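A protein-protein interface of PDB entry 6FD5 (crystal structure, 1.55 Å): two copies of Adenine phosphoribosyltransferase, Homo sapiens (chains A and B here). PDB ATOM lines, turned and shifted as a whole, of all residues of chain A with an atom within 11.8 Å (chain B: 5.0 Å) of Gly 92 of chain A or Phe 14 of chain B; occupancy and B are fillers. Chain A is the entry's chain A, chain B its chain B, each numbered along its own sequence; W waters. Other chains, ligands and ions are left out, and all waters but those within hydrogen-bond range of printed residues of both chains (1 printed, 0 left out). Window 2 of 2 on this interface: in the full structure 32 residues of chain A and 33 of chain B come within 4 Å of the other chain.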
ATOM      1  N   LEU A  83     -12.209 -22.203  -3.799  1.00  0.00           N
ATOM      2  CA  LEU A  83     -10.888 -22.808  -3.822  1.00  0.00           C
ATOM      3  C   LEU A  83      -9.866 -21.914  -3.153  1.00  0.00           C
ATOM      4  O   LEU A  83      -9.837 -20.703  -3.403  1.00  0.00           O
ATOM      5  CB  LEU A  83     -10.429 -23.021  -5.262  1.00  0.00           C
ATOM      6  CG  LEU A  83     -11.294 -23.867  -6.193  1.00  0.00           C
ATOM      7  CD1 LEU A  83     -10.613 -23.982  -7.553  1.00  0.00           C
ATOM      8  CD2 LEU A  83     -11.565 -25.229  -5.580  1.00  0.00           C
ATOM      9  N   ARG A  85      -5.749 -21.891  -3.074  1.00  0.00           N
ATOM     10  CA  ARG A  85      -4.686 -22.577  -3.826  1.00  0.00           C
ATOM     11  C   ARG A  85      -3.295 -22.218  -3.353  1.00  0.00           C
ATOM     12  O   ARG A  85      -3.070 -21.184  -2.720  1.00  0.00           O
ATOM     13  CB  ARG A  85      -4.812 -22.289  -5.316  1.00  0.00           C
ATOM     14  CG  ARG A  85      -6.094 -22.836  -5.922  1.00  0.00           C
ATOM     15  CD  ARG A  85      -5.866 -23.462  -7.286  1.00  0.00           C
ATOM     16  NE  ARG A  85      -4.906 -24.563  -7.191  1.00  0.00           N
ATOM     17  CZ  ARG A  85      -4.405 -25.229  -8.231  1.00  0.00           C
ATOM     18  NH1 ARG A  85      -4.770 -24.920  -9.473  1.00  0.00           N
ATOM     19  NH2 ARG A  85      -3.506 -26.185  -8.032  1.00  0.00           N
ATOM     20  N   LYS A  86      -2.328 -23.046  -3.720  1.00  0.00           N
ATOM     21  CA  LYS A  86      -0.931 -22.645  -3.630  1.00  0.00           C
ATOM     22  C   LYS A  86      -0.691 -21.438  -4.546  1.00  0.00           C
ATOM     23  O   LYS A  86      -1.291 -21.311  -5.616  1.00  0.00           O
ATOM     24  CB  LYS A  86      -0.035 -23.830  -3.990  1.00  0.00           C
ATOM     25  CG  LYS A  86      -0.317 -25.063  -3.149  1.00  0.00           C
ATOM     26  CD  LYS A  86       0.391 -25.020  -1.810  1.00  0.00           C
ATOM     27  CE  LYS A  86       0.274 -26.342  -1.068  1.00  0.00           C
ATOM     28  NZ  LYS A  86      -1.037 -26.469  -0.382  1.00  0.00           N
ATOM     29  N   ARG A  87       0.113 -20.497  -4.074  1.00  0.00           N
ATOM     30  CA  ARG A  87       0.352 -19.282  -4.832  1.00  0.00           C
ATOM     31  C   ARG A  87       0.840 -19.512  -6.261  1.00  0.00           C
ATOM     32  O   ARG A  87       1.684 -20.373  -6.527  1.00  0.00           O
ATOM     33  CB  ARG A  87       1.318 -18.369  -4.103  1.00  0.00           C
ATOM     34  CG  ARG A  87       1.515 -17.088  -4.863  1.00  0.00           C
ATOM     35  CD  ARG A  87       1.982 -15.971  -3.982  1.00  0.00           C
ATOM     36  NE  ARG A  87       2.158 -14.774  -4.786  1.00  0.00           N
ATOM     37  CZ  ARG A  87       3.081 -13.852  -4.549  1.00  0.00           C
ATOM     38  NH1 ARG A  87       3.178 -12.789  -5.338  1.00  0.00           N
ATOM     39  NH2 ARG A  87       3.906 -14.001  -3.522  1.00  0.00           N
ATOM     40  N   GLY A  88       0.300 -18.721  -7.176  1.00  0.00           N
ATOM     41  CA  GLY A  88       0.712 -18.745  -8.568  1.00  0.00           C
ATOM     42  C   GLY A  88      -0.230 -19.483  -9.500  1.00  0.00           C
ATOM     43  O   GLY A  88      -0.029 -19.460 -10.719  1.00  0.00           O
ATOM     44  N   LYS A  89      -1.278 -20.089  -8.941  1.00  0.00           N
ATOM     45  CA  LYS A  89      -2.161 -20.964  -9.707  1.00  0.00           C
ATOM     46  C   LYS A  89      -3.442 -20.276 -10.201  1.00  0.00           C
ATOM     47  O   LYS A  89      -4.068 -20.722 -11.159  1.00  0.00           O
ATOM     48  CB  LYS A  89      -2.530 -22.180  -8.856  1.00  0.00           C
ATOM     49  CG  LYS A  89      -1.338 -22.995  -8.366  1.00  0.00           C
ATOM     50  CD  LYS A  89      -0.761 -23.864  -9.461  1.00  0.00           C
ATOM     51  CE  LYS A  89       0.071 -25.001  -8.879  1.00  0.00           C
ATOM     52  NZ  LYS A  89       0.430 -26.010  -9.919  1.00  0.00           N
ATOM     53  N   LEU A  90      -3.856 -19.215  -9.522  1.00  0.00           N
ATOM     54  CA  LEU A  90      -5.145 -18.585  -9.805  1.00  0.00           C
ATOM     55  C   LEU A  90      -5.014 -17.335 -10.652  1.00  0.00           C
ATOM     56  O   LEU A  90      -4.114 -16.504 -10.424  1.00  0.00           O
ATOM     57  CB  LEU A  90      -5.826 -18.184  -8.504  1.00  0.00           C
ATOM     58  CG  LEU A  90      -6.312 -19.321  -7.618  1.00  0.00           C
ATOM     59  CD1 LEU A  90      -6.647 -18.769  -6.248  1.00  0.00           C
ATOM     60  CD2 LEU A  90      -7.508 -20.023  -8.242  1.00  0.00           C
ATOM     61  N   PRO A  91      -5.951 -17.155 -11.600  1.00  0.00           N
ATOM     62  CA  PRO A  91      -6.006 -15.950 -12.394  1.00  0.00           C
ATOM     63  C   PRO A  91      -6.760 -14.833 -11.683  1.00  0.00           C
ATOM     64  O   PRO A  91      -7.452 -15.088 -10.691  1.00  0.00           O
ATOM     65  CB  PRO A  91      -6.809 -16.397 -13.626  1.00  0.00           C
ATOM     66  CG  PRO A  91      -7.774 -17.376 -13.056  1.00  0.00           C
ATOM     67  CD  PRO A  91      -6.964 -18.140 -12.030  1.00  0.00           C
ATOM     68  N   GLY A  92      -6.607 -13.615 -12.194  1.00  0.00           N
ATOM     69  CA  GLY A  92      -7.282 -12.457 -11.608  1.00  0.00           C
ATOM     70  C   GLY A  92      -6.592 -11.954 -10.350  1.00  0.00           C
ATOM     71  O   GLY A  92      -5.596 -12.523  -9.886  1.00  0.00           O
ATOM     72  N   PRO A  93      -7.135 -10.885  -9.766  1.00  0.00           N
ATOM     73  CA  PRO A  93      -6.525 -10.304  -8.567  1.00  0.00           C
ATOM     74  C   PRO A  93      -6.619 -11.261  -7.385  1.00  0.00           C
ATOM     75  O   PRO A  93      -7.650 -11.902  -7.184  1.00  0.00           O
ATOM     76  CB  PRO A  93      -7.379  -9.064  -8.315  1.00  0.00           C
ATOM     77  CG  PRO A  93      -7.926  -8.715  -9.664  1.00  0.00           C
ATOM     78  CD  PRO A  93      -8.208 -10.035 -10.307  1.00  0.00           C
ATOM     79  N   THR A  94      -5.516 -11.383  -6.645  1.00  0.00           N
ATOM     80  CA  THR A  94      -5.465 -12.330  -5.533  1.00  0.00           C
ATOM     81  C   THR A  94      -4.918 -11.696  -4.277  1.00  0.00           C
ATOM     82  O   THR A  94      -4.309 -10.629  -4.312  1.00  0.00           O
ATOM     83  CB  THR A  94      -4.586 -13.555  -5.835  1.00  0.00           C
ATOM     84  OG1 THR A  94      -3.249 -13.126  -6.100  1.00  0.00           O
ATOM     85  CG2 THR A  94      -5.132 -14.329  -7.055  1.00  0.00           C
ATOM     86  N   LEU A  95      -5.189 -12.370  -3.164  1.00  0.00           N
ATOM     87  CA  LEU A  95      -4.491 -12.133  -1.904  1.00  0.00           C
ATOM     88  C   LEU A  95      -3.725 -13.394  -1.562  1.00  0.00           C
ATOM     89  O   LEU A  95      -4.148 -14.477  -1.945  1.00  0.00           O
ATOM     90  CB  LEU A  95      -5.503 -11.882  -0.785  1.00  0.00           C
ATOM     91  CG  LEU A  95      -6.601 -10.852  -0.991  1.00  0.00           C
ATOM     92  CD1 LEU A  95      -7.427 -10.777   0.278  1.00  0.00           C
ATOM     93  CD2 LEU A  95      -5.990  -9.494  -1.338  1.00  0.00           C
ATOM     94  N   TRP A  96      -2.656 -13.274  -0.781  1.00  0.00           N
ATOM     95  CA  TRP A  96      -1.883 -14.455  -0.394  1.00  0.00           C
ATOM     96  C   TRP A  96      -1.370 -14.352   1.040  1.00  0.00           C
ATOM     97  O   TRP A  96      -1.320 -13.265   1.622  1.00  0.00           O
ATOM     98  CB  TRP A  96      -0.739 -14.736  -1.384  1.00  0.00           C
ATOM     99  CG  TRP A  96       0.265 -13.643  -1.540  1.00  0.00           C
ATOM    100  CD1 TRP A  96       1.399 -13.445  -0.806  1.00  0.00           C
ATOM    101  CD2 TRP A  96       0.256 -12.629  -2.543  1.00  0.00           C
ATOM    102  NE1 TRP A  96       2.067 -12.327  -1.253  1.00  0.00           N
ATOM    103  CE2 TRP A  96       1.397 -11.822  -2.334  1.00  0.00           C
ATOM    104  CE3 TRP A  96      -0.623 -12.305  -3.578  1.00  0.00           C
ATOM    105  CZ2 TRP A  96       1.681 -10.719  -3.128  1.00  0.00           C
ATOM    106  CZ3 TRP A  96      -0.332 -11.224  -4.374  1.00  0.00           C
ATOM    107  CH2 TRP A  96       0.810 -10.442  -4.146  1.00  0.00           C
ATOM    108  N   LEU A 108      -0.355 -19.637   0.421  1.00  0.00           N
ATOM    109  CA  LEU A 108      -1.683 -19.905  -0.139  1.00  0.00           C
ATOM    110  C   LEU A 108      -2.276 -18.614  -0.702  1.00  0.00           C
ATOM    111  O   LEU A 108      -1.845 -17.518  -0.340  1.00  0.00           O
ATOM    112  CB  LEU A 108      -2.633 -20.438   0.930  1.00  0.00           C
ATOM    113  CG  LEU A 108      -2.350 -21.830   1.503  1.00  0.00           C
ATOM    114  CD1 LEU A 108      -3.446 -22.212   2.488  1.00  0.00           C
ATOM    115  CD2 LEU A 108      -2.249 -22.879   0.420  1.00  0.00           C
ATOM    116  N   GLU A 109      -3.241 -18.754  -1.604  1.00  0.00           N
ATOM    117  CA  GLU A 109      -3.825 -17.596  -2.269  1.00  0.00           C
ATOM    118  C   GLU A 109      -5.311 -17.833  -2.496  1.00  0.00           C
ATOM    119  O   GLU A 109      -5.771 -18.977  -2.591  1.00  0.00           O
ATOM    120  CB  GLU A 109      -3.139 -17.313  -3.619  1.00  0.00           C
ATOM    121  CG  GLU A 109      -3.242 -18.469  -4.599  1.00  0.00           C
ATOM    122  CD  GLU A 109      -2.807 -18.127  -6.024  1.00  0.00           C
ATOM    123  OE1 GLU A 109      -2.026 -17.163  -6.223  1.00  0.00           O
ATOM    124  OE2 GLU A 109      -3.213 -18.886  -6.939  1.00  0.00           O
ATOM    125  N   ILE A 110      -6.040 -16.735  -2.623  1.00  0.00           N
ATOM    126  CA  ILE A 110      -7.461 -16.764  -2.936  1.00  0.00           C
ATOM    127  C   ILE A 110      -7.779 -15.582  -3.852  1.00  0.00           C
ATOM    128  O   ILE A 110      -7.107 -14.536  -3.791  1.00  0.00           O
ATOM    129  CB  ILE A 110      -8.301 -16.692  -1.648  1.00  0.00           C
ATOM    130  CG1 ILE A 110      -9.760 -17.069  -1.903  1.00  0.00           C
ATOM    131  CG2 ILE A 110      -8.206 -15.325  -0.998  1.00  0.00           C
ATOM    132  CD1 ILE A 110     -10.532 -17.331  -0.613  1.00  0.00           C
ATOM    133  N   GLN A 111      -8.772 -15.744  -4.732  1.00  0.00           N
ATOM    134  CA  GLN A 111      -9.203 -14.627  -5.579  1.00  0.00           C
ATOM    135  C   GLN A 111      -9.905 -13.579  -4.720  1.00  0.00           C
ATOM    136  O   GLN A 111     -10.677 -13.909  -3.809  1.00  0.00           O
ATOM    137  CB  GLN A 111     -10.110 -15.109  -6.727  1.00  0.00           C
ATOM    138  CG  GLN A 111      -9.355 -15.930  -7.774  1.00  0.00           C
ATOM    139  CD  GLN A 111     -10.258 -16.658  -8.786  1.00  0.00           C
ATOM    140  OE1 GLN A 111     -11.381 -17.071  -8.485  1.00  0.00           O
ATOM    141  NE2 GLN A 111      -9.780 -16.750 -10.014  1.00  0.00           N
ATOM    142  N   LYS A 112      -9.637 -12.314  -5.019  1.00  0.00           N
ATOM    143  CA  LYS A 112     -10.231 -11.213  -4.267  1.00  0.00           C
ATOM    144  C   LYS A 112     -11.748 -11.239  -4.327  1.00  0.00           C
ATOM    145  O   LYS A 112     -12.401 -10.710  -3.429  1.00  0.00           O
ATOM    146  CB  LYS A 112      -9.749  -9.860  -4.783  1.00  0.00           C
ATOM    147  CG  LYS A 112      -8.283  -9.558  -4.529  1.00  0.00           C
ATOM    148  CD  LYS A 112      -7.998  -8.073  -4.675  1.00  0.00           C
ATOM    149  CE  LYS A 112      -6.510  -7.750  -4.634  1.00  0.00           C
ATOM    150  NZ  LYS A 112      -6.262  -6.288  -4.764  1.00  0.00           N
ATOM    151  N   ASP A 113     -12.311 -11.823  -5.384  1.00  0.00           N
ATOM    152  CA  ASP A 113     -13.772 -11.874  -5.520  1.00  0.00           C
ATOM    153  C   ASP A 113     -14.379 -13.238  -5.195  1.00  0.00           C
ATOM    154  O   ASP A 113     -15.519 -13.518  -5.560  1.00  0.00           O
ATOM    155  CB  ASP A 113     -14.194 -11.403  -6.920  1.00  0.00           C
ATOM    156  CG  ASP A 113     -13.844 -12.391  -8.015  1.00  0.00           C
ATOM    157  OD1 ASP A 113     -13.151 -13.398  -7.754  1.00  0.00           O
ATOM    158  OD2 ASP A 113     -14.280 -12.144  -9.162  1.00  0.00           O
ATOM    159  N   ALA A 114     -13.650 -14.059  -4.445  1.00  0.00           N
ATOM    160  CA  ALA A 114     -14.119 -15.414  -4.130  1.00  0.00           C
ATOM    161  C   ALA A 114     -15.378 -15.409  -3.246  1.00  0.00           C
ATOM    162  O   ALA A 114     -16.233 -16.292  -3.374  1.00  0.00           O
ATOM    163  CB  ALA A 114     -13.023 -16.207  -3.447  1.00  0.00           C
ATOM    164  N   LEU A 144     -11.157 -11.169   3.308  1.00  0.00           N
ATOM    165  CA  LEU A 144     -12.345 -10.933   2.479  1.00  0.00           C
ATOM    166  C   LEU A 144     -13.572 -10.614   3.317  1.00  0.00           C
ATOM    167  O   LEU A 144     -14.672 -10.459   2.782  1.00  0.00           O
ATOM    168  CB  LEU A 144     -12.654 -12.152   1.622  1.00  0.00           C
ATOM    169  CG  LEU A 144     -11.541 -12.513   0.648  1.00  0.00           C
ATOM    170  CD1 LEU A 144     -11.946 -13.745  -0.149  1.00  0.00           C
ATOM    171  CD2 LEU A 144     -11.225 -11.321  -0.246  1.00  0.00           C
ATOM    172  N   ARG B  12     -15.130 -18.963 -16.870  1.00  0.00           N
ATOM    173  CA  ARG B  12     -14.710 -17.576 -16.926  1.00  0.00           C
ATOM    174  C   ARG B  12     -13.324 -17.523 -17.573  1.00  0.00           C
ATOM    175  O   ARG B  12     -12.457 -18.335 -17.249  1.00  0.00           O
ATOM    176  CB  ARG B  12     -14.658 -17.014 -15.497  1.00  0.00           C
ATOM    177  CG  ARG B  12     -14.303 -15.551 -15.409  1.00  0.00           C
ATOM    178  CD  ARG B  12     -14.433 -15.041 -13.984  1.00  0.00           C
ATOM    179  NE  ARG B  12     -13.864 -15.966 -13.014  1.00  0.00           N
ATOM    180  CZ  ARG B  12     -13.754 -15.718 -11.717  1.00  0.00           C
ATOM    181  NH1 ARG B  12     -14.162 -14.553 -11.226  1.00  0.00           N
ATOM    182  NH2 ARG B  12     -13.243 -16.640 -10.908  1.00  0.00           N
ATOM    183  N   SER B  13     -13.141 -16.629 -18.542  1.00  0.00           N
ATOM    184  CA  SER B  13     -11.913 -16.591 -19.326  1.00  0.00           C
ATOM    185  C   SER B  13     -11.064 -15.363 -18.990  1.00  0.00           C
ATOM    186  O   SER B  13     -11.560 -14.228 -18.945  1.00  0.00           O
ATOM    187  CB  SER B  13     -12.248 -16.613 -20.814  1.00  0.00           C
ATOM    188  OG  SER B  13     -12.803 -17.863 -21.162  1.00  0.00           O
ATOM    189  N   PHE B  14      -9.784 -15.596 -18.710  1.00  0.00           N
ATOM    190  CA  PHE B  14      -8.864 -14.528 -18.338  1.00  0.00           C
ATOM    191  C   PHE B  14      -7.748 -14.394 -19.368  1.00  0.00           C
ATOM    192  O   PHE B  14      -6.900 -15.279 -19.472  1.00  0.00           O
ATOM    193  CB  PHE B  14      -8.229 -14.835 -16.981  1.00  0.00           C
ATOM    194  CG  PHE B  14      -9.154 -14.646 -15.817  1.00  0.00           C
ATOM    195  CD1 PHE B  14      -9.244 -13.407 -15.194  1.00  0.00           C
ATOM    196  CD2 PHE B  14      -9.918 -15.710 -15.327  1.00  0.00           C
ATOM    197  CE1 PHE B  14     -10.081 -13.233 -14.094  1.00  0.00           C
ATOM    198  CE2 PHE B  14     -10.762 -15.529 -14.253  1.00  0.00           C
ATOM    199  CZ  PHE B  14     -10.826 -14.298 -13.631  1.00  0.00           C
ATOM    200  N   PRO B  15      -7.738 -13.296 -20.124  1.00  0.00           N
ATOM    201  CA  PRO B  15      -6.666 -13.119 -21.096  1.00  0.00           C
ATOM    202  C   PRO B  15      -5.315 -12.878 -20.441  1.00  0.00           C
ATOM    203  O   PRO B  15      -5.230 -12.314 -19.350  1.00  0.00           O
ATOM    204  CB  PRO B  15      -7.105 -11.893 -21.885  1.00  0.00           C
ATOM    205  CG  PRO B  15      -7.915 -11.105 -20.914  1.00  0.00           C
ATOM    206  CD  PRO B  15      -8.601 -12.104 -20.035  1.00  0.00           C
ATOM    207  N   ASP B  16      -4.260 -13.319 -21.116  1.00  0.00           N
ATOM    208  CA  ASP B  16      -2.894 -12.972 -20.742  1.00  0.00           C
ATOM    209  C   ASP B  16      -2.490 -13.523 -19.373  1.00  0.00           C
ATOM    210  O   ASP B  16      -1.653 -12.935 -18.693  1.00  0.00           O
ATOM    211  CB  ASP B  16      -2.686 -11.455 -20.824  1.00  0.00           C
ATOM    212  CG  ASP B  16      -3.067 -10.886 -22.192  1.00  0.00           C
ATOM    213  OD1 ASP B  16      -2.736 -11.515 -23.222  1.00  0.00           O
ATOM    214  OD2 ASP B  16      -3.711  -9.815 -22.253  1.00  0.00           O
ATOM    215  N   PHE B  17      -3.041 -14.679 -19.022  1.00  0.00           N
ATOM    216  CA  PHE B  17      -2.630 -15.434 -17.831  1.00  0.00           C
ATOM    217  C   PHE B  17      -2.360 -16.891 -18.207  1.00  0.00           C
ATOM    218  O   PHE B  17      -3.223 -17.536 -18.795  1.00  0.00           O
ATOM    219  CB  PHE B  17      -3.703 -15.379 -16.736  1.00  0.00           C
ATOM    220  CG  PHE B  17      -3.286 -16.044 -15.452  1.00  0.00           C
ATOM    221  CD1 PHE B  17      -2.556 -15.348 -14.507  1.00  0.00           C
ATOM    222  CD2 PHE B  17      -3.551 -17.377 -15.236  1.00  0.00           C
ATOM    223  CE1 PHE B  17      -2.128 -15.967 -13.349  1.00  0.00           C
ATOM    224  CE2 PHE B  17      -3.134 -18.010 -14.075  1.00  0.00           C
ATOM    225  CZ  PHE B  17      -2.415 -17.298 -13.131  1.00  0.00           C
ATOM    226  N   VAL B  22      -2.270 -15.855 -24.193  1.00  0.00           N
ATOM    227  CA  VAL B  22      -3.068 -17.017 -23.842  1.00  0.00           C
ATOM    228  C   VAL B  22      -4.313 -16.636 -23.060  1.00  0.00           C
ATOM    229  O   VAL B  22      -4.360 -15.605 -22.392  1.00  0.00           O
ATOM    230  CB  VAL B  22      -2.245 -18.032 -23.027  1.00  0.00           C
ATOM    231  CG1 VAL B  22      -1.666 -17.392 -21.784  1.00  0.00           C
ATOM    232  CG2 VAL B  22      -3.081 -19.242 -22.654  1.00  0.00           C
ATOM    233  N   VAL B  23      -5.314 -17.500 -23.129  1.00  0.00           N
ATOM    234  CA  VAL B  23      -6.526 -17.293 -22.379  1.00  0.00           C
ATOM    235  C   VAL B  23      -6.688 -18.426 -21.386  1.00  0.00           C
ATOM    236  O   VAL B  23      -6.786 -19.594 -21.770  1.00  0.00           O
ATOM    237  CB  VAL B  23      -7.746 -17.226 -23.309  1.00  0.00           C
ATOM    238  CG1 VAL B  23      -9.016 -16.969 -22.514  1.00  0.00           C
ATOM    239  CG2 VAL B  23      -7.546 -16.149 -24.355  1.00  0.00           C
ATOM    240  N   PHE B  24      -6.737 -18.074 -20.106  1.00  0.00           N
ATOM    241  CA  PHE B  24      -6.945 -19.040 -19.048  1.00  0.00           C
ATOM    242  C   PHE B  24      -8.438 -19.322 -18.861  1.00  0.00           C
ATOM    243  O   PHE B  24      -9.242 -18.415 -18.693  1.00  0.00           O
ATOM    244  CB  PHE B  24      -6.322 -18.527 -17.749  1.00  0.00           C
ATOM    245  CG  PHE B  24      -6.256 -19.557 -16.659  1.00  0.00           C
ATOM    246  CD1 PHE B  24      -7.336 -19.778 -15.820  1.00  0.00           C
ATOM    247  CD2 PHE B  24      -5.101 -20.300 -16.458  1.00  0.00           C
ATOM    248  CE1 PHE B  24      -7.283 -20.730 -14.814  1.00  0.00           C
ATOM    249  CE2 PHE B  24      -5.040 -21.256 -15.454  1.00  0.00           C
ATOM    250  CZ  PHE B  24      -6.127 -21.463 -14.623  1.00  0.00           C
ATOM    251  N   ASP B  26     -11.082 -20.580 -16.478  1.00  0.00           N
ATOM    252  CA  ASP B  26     -11.234 -20.750 -15.025  1.00  0.00           C
ATOM    253  C   ASP B  26     -12.527 -21.504 -14.745  1.00  0.00           C
ATOM    254  O   ASP B  26     -13.620 -21.017 -15.064  1.00  0.00           O
ATOM    255  CB  ASP B  26     -11.237 -19.387 -14.343  1.00  0.00           C
ATOM    256  CG  ASP B  26     -11.338 -19.469 -12.822  1.00  0.00           C
ATOM    257  OD1 ASP B  26     -11.064 -20.543 -12.243  1.00  0.00           O
ATOM    258  OD2 ASP B  26     -11.684 -18.420 -12.224  1.00  0.00           O
HETATM  259  O   HOH W   1     -13.683 -16.061  -7.607  1.00  0.00           O
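Of the printed residues of chain B, Leu 90 of chain A touches Phe 17.
Printed residues of chain B within 4 Å of Pro 91 of chain A: Phe 14 (3.5 Å), Phe 17 (3.8 Å) and Phe 24 (3.7 Å).
Trp 96 of chain A touches none of the printed residues of chain B.
Glu 109 of chain A touches none of the printed residues of chain B.
Of the printed residues of chain B, Gln 111 of chain A touches Arg 12 and Asp 26.
Of the printed residues of chain B, Asp 113 of chain A touches Arg 12 (3.2 Å).
Arg 12 of chain B touches two residues of chain A.
No residue of chain A comes within 4 Å of Ser 13 of chain B.
Phe 14 of chain B touches just these residues of chain A: Pro 91 and Gly 92.
No residue of chain A comes within 4 Å of Pro 15 of chain B.
No residue of chain A comes within 4 Å of Asp 16 of chain B.
Of chain A, only Leu 90 and Pro 91 come within 4 Å of Phe 17 of chain B.
Of chain A, only Pro 91 (3.7 Å) comes within 4 Å of Phe 24 of chain B.
Asp 26 of chain B touches just one residue of chain A: Gln 111 (3.4 Å).
The nearest printed residue of chain B that does not touch Gly 92 of chain A is Phe 17 of chain B (5.0 Å).
The nearest residue of chain A that does not touch Phe 14 of chain B is Gln 111 of chain A (4.5 Å).
The nearest printed residue of chain B that does not touch Asp 113 of chain A is Phe 14 of chain B (6.0 Å).
Among the printed residues, pairs that only touch across the chains: Leu 90 of chain A with Phe 17 of chain B (3.3 Å), Pro 91 of chain A with Phe 14 of chain B (3.5 Å), Pro 91 of chain A with Phe 24 of chain B (3.7 Å), Pro 91 of chain A with Phe 17 of chain B (3.8 Å) and Gly 92 of chain A with Phe 14 of chain B (3.8 Å).
The backbone NH (N) of Phe 14 of chain B sits at hydrogen-bond distance from the backbone carbonyl oxygen (O) of Phe 24 of chain B (2.9 Å).
The guanidinium group (NH2) of Arg 12 of chain B is in salt-bridge range of the side-chain carboxylate (OD2) of Asp 26 of chain B (2.7 Å).
The side-chain amide nitrogen (NE2) of Gln 111 of chain A sits at hydrogen-bond distance from the backbone carbonyl oxygen (O) of Pro 91 of chain A (2.9 Å).
N of Leu 90 of chain A is in hydrogen-bond range of OE2 of Glu 109 of chain A, at 2.7 Å.
No position is printed for both chains.
Water W1 lies within hydrogen-bond range of the side-chain amide oxygen of Gln 111 of chain A (2.7 Å), the side-chain carboxylate of Asp 113 of chain A (2.7 Å) and the guanidinium group of Arg 12 of chain B (3.4 Å).
Of the 21 printed residues of chain A, 5 touch a printed residue of chain B.
Hydrophobic or aromatic side chains of chain B within 4 Å of the printed part of chain A: Phe 14, Phe 17 and Phe 24.
Among the printed residues, Asp or Glu carboxylates within 4 Å of a Lys or Arg side-chain nitrogen of the other chain: Asp 113 of chain A with Arg 12 of chain B (3.2 Å).
The side-chain carboxylate (OD2) of Asp 26 of chain B lies within hydrogen-bond range of the side-chain amide nitrogen (NE2) of Gln 111 of chain A (3.4 Å).
OE1 of Gln 111 of chain A sits at hydrogen-bond distance from NH2 of Arg 12 of chain B, at 3.1 Å.
The side-chain carboxylate (OD2) of Asp 113 of chain A is in salt-bridge range of the guanidinium group (NH1) of Arg 12 of chain B (3.2 Å).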
